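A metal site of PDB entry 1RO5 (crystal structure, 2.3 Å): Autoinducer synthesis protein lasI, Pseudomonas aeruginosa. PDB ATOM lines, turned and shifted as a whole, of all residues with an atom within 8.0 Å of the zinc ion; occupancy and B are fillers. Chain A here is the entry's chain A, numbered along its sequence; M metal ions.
The zinc ion is bound by ND1 of His 3 (1.8 Å), N of Ser 2 (1.9 Å), N of His 3 (2.1 Å) and N of Gly 1 (2.1 Å).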
ATOM      1  N   GLY A   1     -10.099 -18.846  -0.269  1.00  0.00           N
ATOM      2  CA  GLY A   1     -11.038 -18.050  -1.158  1.00  0.00           C
ATOM      3  C   GLY A   1     -12.310 -18.767  -1.604  1.00  0.00           C
ATOM      4  O   GLY A   1     -13.245 -18.070  -2.156  1.00  0.00           O
ATOM      5  N   SER A   2     -12.355 -20.112  -1.397  1.00  0.00           N
ATOM      6  CA  SER A   2     -13.535 -20.984  -1.729  1.00  0.00           C
ATOM      7  C   SER A   2     -13.156 -22.398  -1.384  1.00  0.00           C
ATOM      8  O   SER A   2     -13.892 -23.346  -1.640  1.00  0.00           O
ATOM      9  CB  SER A   2     -13.966 -20.945  -3.234  1.00  0.00           C
ATOM     10  OG  SER A   2     -14.236 -19.620  -3.664  1.00  0.00           O
ATOM     11  N   HIS A   3     -11.968 -22.541  -0.876  1.00  0.00           N
ATOM     12  CA  HIS A   3     -11.500 -23.824  -0.445  1.00  0.00           C
ATOM     13  C   HIS A   3     -11.806 -24.074   1.085  1.00  0.00           C
ATOM     14  O   HIS A   3     -12.295 -23.189   1.779  1.00  0.00           O
ATOM     15  CB  HIS A   3     -10.000 -23.953  -0.744  1.00  0.00           C
ATOM     16  CG  HIS A   3      -9.154 -23.105   0.101  1.00  0.00           C
ATOM     17  ND1 HIS A   3      -9.365 -21.736   0.194  1.00  0.00           N
ATOM     18  CD2 HIS A   3      -8.083 -23.403   0.905  1.00  0.00           C
ATOM     19  CE1 HIS A   3      -8.444 -21.232   1.020  1.00  0.00           C
ATOM     20  NE2 HIS A   3      -7.616 -22.219   1.403  1.00  0.00           N
ATOM     21  N   MET A   4     -11.499 -25.292   1.541  1.00  0.00           N
ATOM     22  CA  MET A   4     -11.606 -25.667   2.925  1.00  0.00           C
ATOM     23  C   MET A   4     -10.302 -25.419   3.681  1.00  0.00           C
ATOM     24  O   MET A   4      -9.173 -25.758   3.169  1.00  0.00           O
ATOM     25  CB  MET A   4     -12.053 -27.114   3.034  1.00  0.00           C
ATOM     26  CG  MET A   4     -13.446 -27.329   2.422  1.00  0.00           C
ATOM     27  SD  MET A   4     -14.181 -28.896   3.205  1.00  0.00           S
ATOM     28  CE  MET A   4     -12.616 -29.516   4.264  1.00  0.00           C
ATOM     29  N   ILE A   5     -10.447 -24.797   4.876  1.00  0.00           N
ATOM     30  CA  ILE A   5      -9.302 -24.569   5.760  1.00  0.00           C
ATOM     31  C   ILE A   5      -9.582 -25.405   6.982  1.00  0.00           C
ATOM     32  O   ILE A   5     -10.715 -25.363   7.554  1.00  0.00           O
ATOM     33  CB  ILE A   5      -9.261 -23.169   6.112  1.00  0.00           C
ATOM     34  CG1 ILE A   5      -8.871 -22.355   4.880  1.00  0.00           C
ATOM     35  CG2 ILE A   5      -8.229 -22.898   7.151  1.00  0.00           C
ATOM     36  CD1 ILE A   5      -9.114 -20.799   5.089  1.00  0.00           C
ATOM     37  N   GLN A  60     -13.144 -24.698   8.186  1.00  0.00           N
ATOM     38  CA  GLN A  60     -13.780 -23.452   7.702  1.00  0.00           C
ATOM     39  C   GLN A  60     -13.981 -23.370   6.197  1.00  0.00           C
ATOM     40  O   GLN A  60     -13.336 -24.050   5.427  1.00  0.00           O
ATOM     41  CB  GLN A  60     -13.011 -22.238   8.150  1.00  0.00           C
ATOM     42  CG  GLN A  60     -12.875 -22.133   9.611  1.00  0.00           C
ATOM     43  CD  GLN A  60     -11.836 -21.095   9.881  1.00  0.00           C
ATOM     44  OE1 GLN A  60     -10.674 -21.444  10.075  1.00  0.00           O
ATOM     45  NE2 GLN A  60     -12.227 -19.796   9.865  1.00  0.00           N
ATOM     46  N   GLU A  61     -14.877 -22.469   5.793  1.00  0.00           N
ATOM     47  CA  GLU A  61     -15.313 -22.345   4.411  1.00  0.00           C
ATOM     48  C   GLU A  61     -16.071 -21.048   4.344  1.00  0.00           C
ATOM     49  O   GLU A  61     -16.926 -20.765   5.211  1.00  0.00           O
ATOM     50  CB  GLU A  61     -16.190 -23.486   4.025  1.00  0.00           C
ATOM     51  CG  GLU A  61     -16.405 -23.528   2.548  1.00  0.00           C
ATOM     52  CD  GLU A  61     -16.644 -24.958   2.047  1.00  0.00           C
ATOM     53  OE1 GLU A  61     -16.423 -25.160   0.808  1.00  0.00           O
ATOM     54  OE2 GLU A  61     -17.053 -25.843   2.856  1.00  0.00           O
ATOM     55  N   ASP A  62     -15.694 -20.232   3.353  1.00  0.00           N
ATOM     56  CA  ASP A  62     -16.199 -18.861   3.176  1.00  0.00           C
ATOM     57  C   ASP A  62     -16.181 -18.025   4.496  1.00  0.00           C
ATOM     58  O   ASP A  62     -17.145 -17.291   4.788  1.00  0.00           O
ATOM     59  CB  ASP A  62     -17.588 -18.854   2.459  1.00  0.00           C
ATOM     60  CG  ASP A  62     -17.658 -19.884   1.243  1.00  0.00           C
ATOM     61  OD1 ASP A  62     -16.651 -20.047   0.427  1.00  0.00           O
ATOM     62  OD2 ASP A  62     -18.682 -20.607   1.019  1.00  0.00           O
ATOM     63  N   GLY A  63     -15.110 -18.216   5.275  1.00  0.00           N
ATOM     64  CA  GLY A  63     -14.793 -17.301   6.373  1.00  0.00           C
ATOM     65  C   GLY A  63     -15.490 -17.677   7.679  1.00  0.00           C
ATOM     66  O   GLY A  63     -15.757 -16.894   8.588  1.00  0.00           O
HETATM   67 ZN    ZN M   1     -10.809 -20.851  -0.522  1.00  0.00          ZN
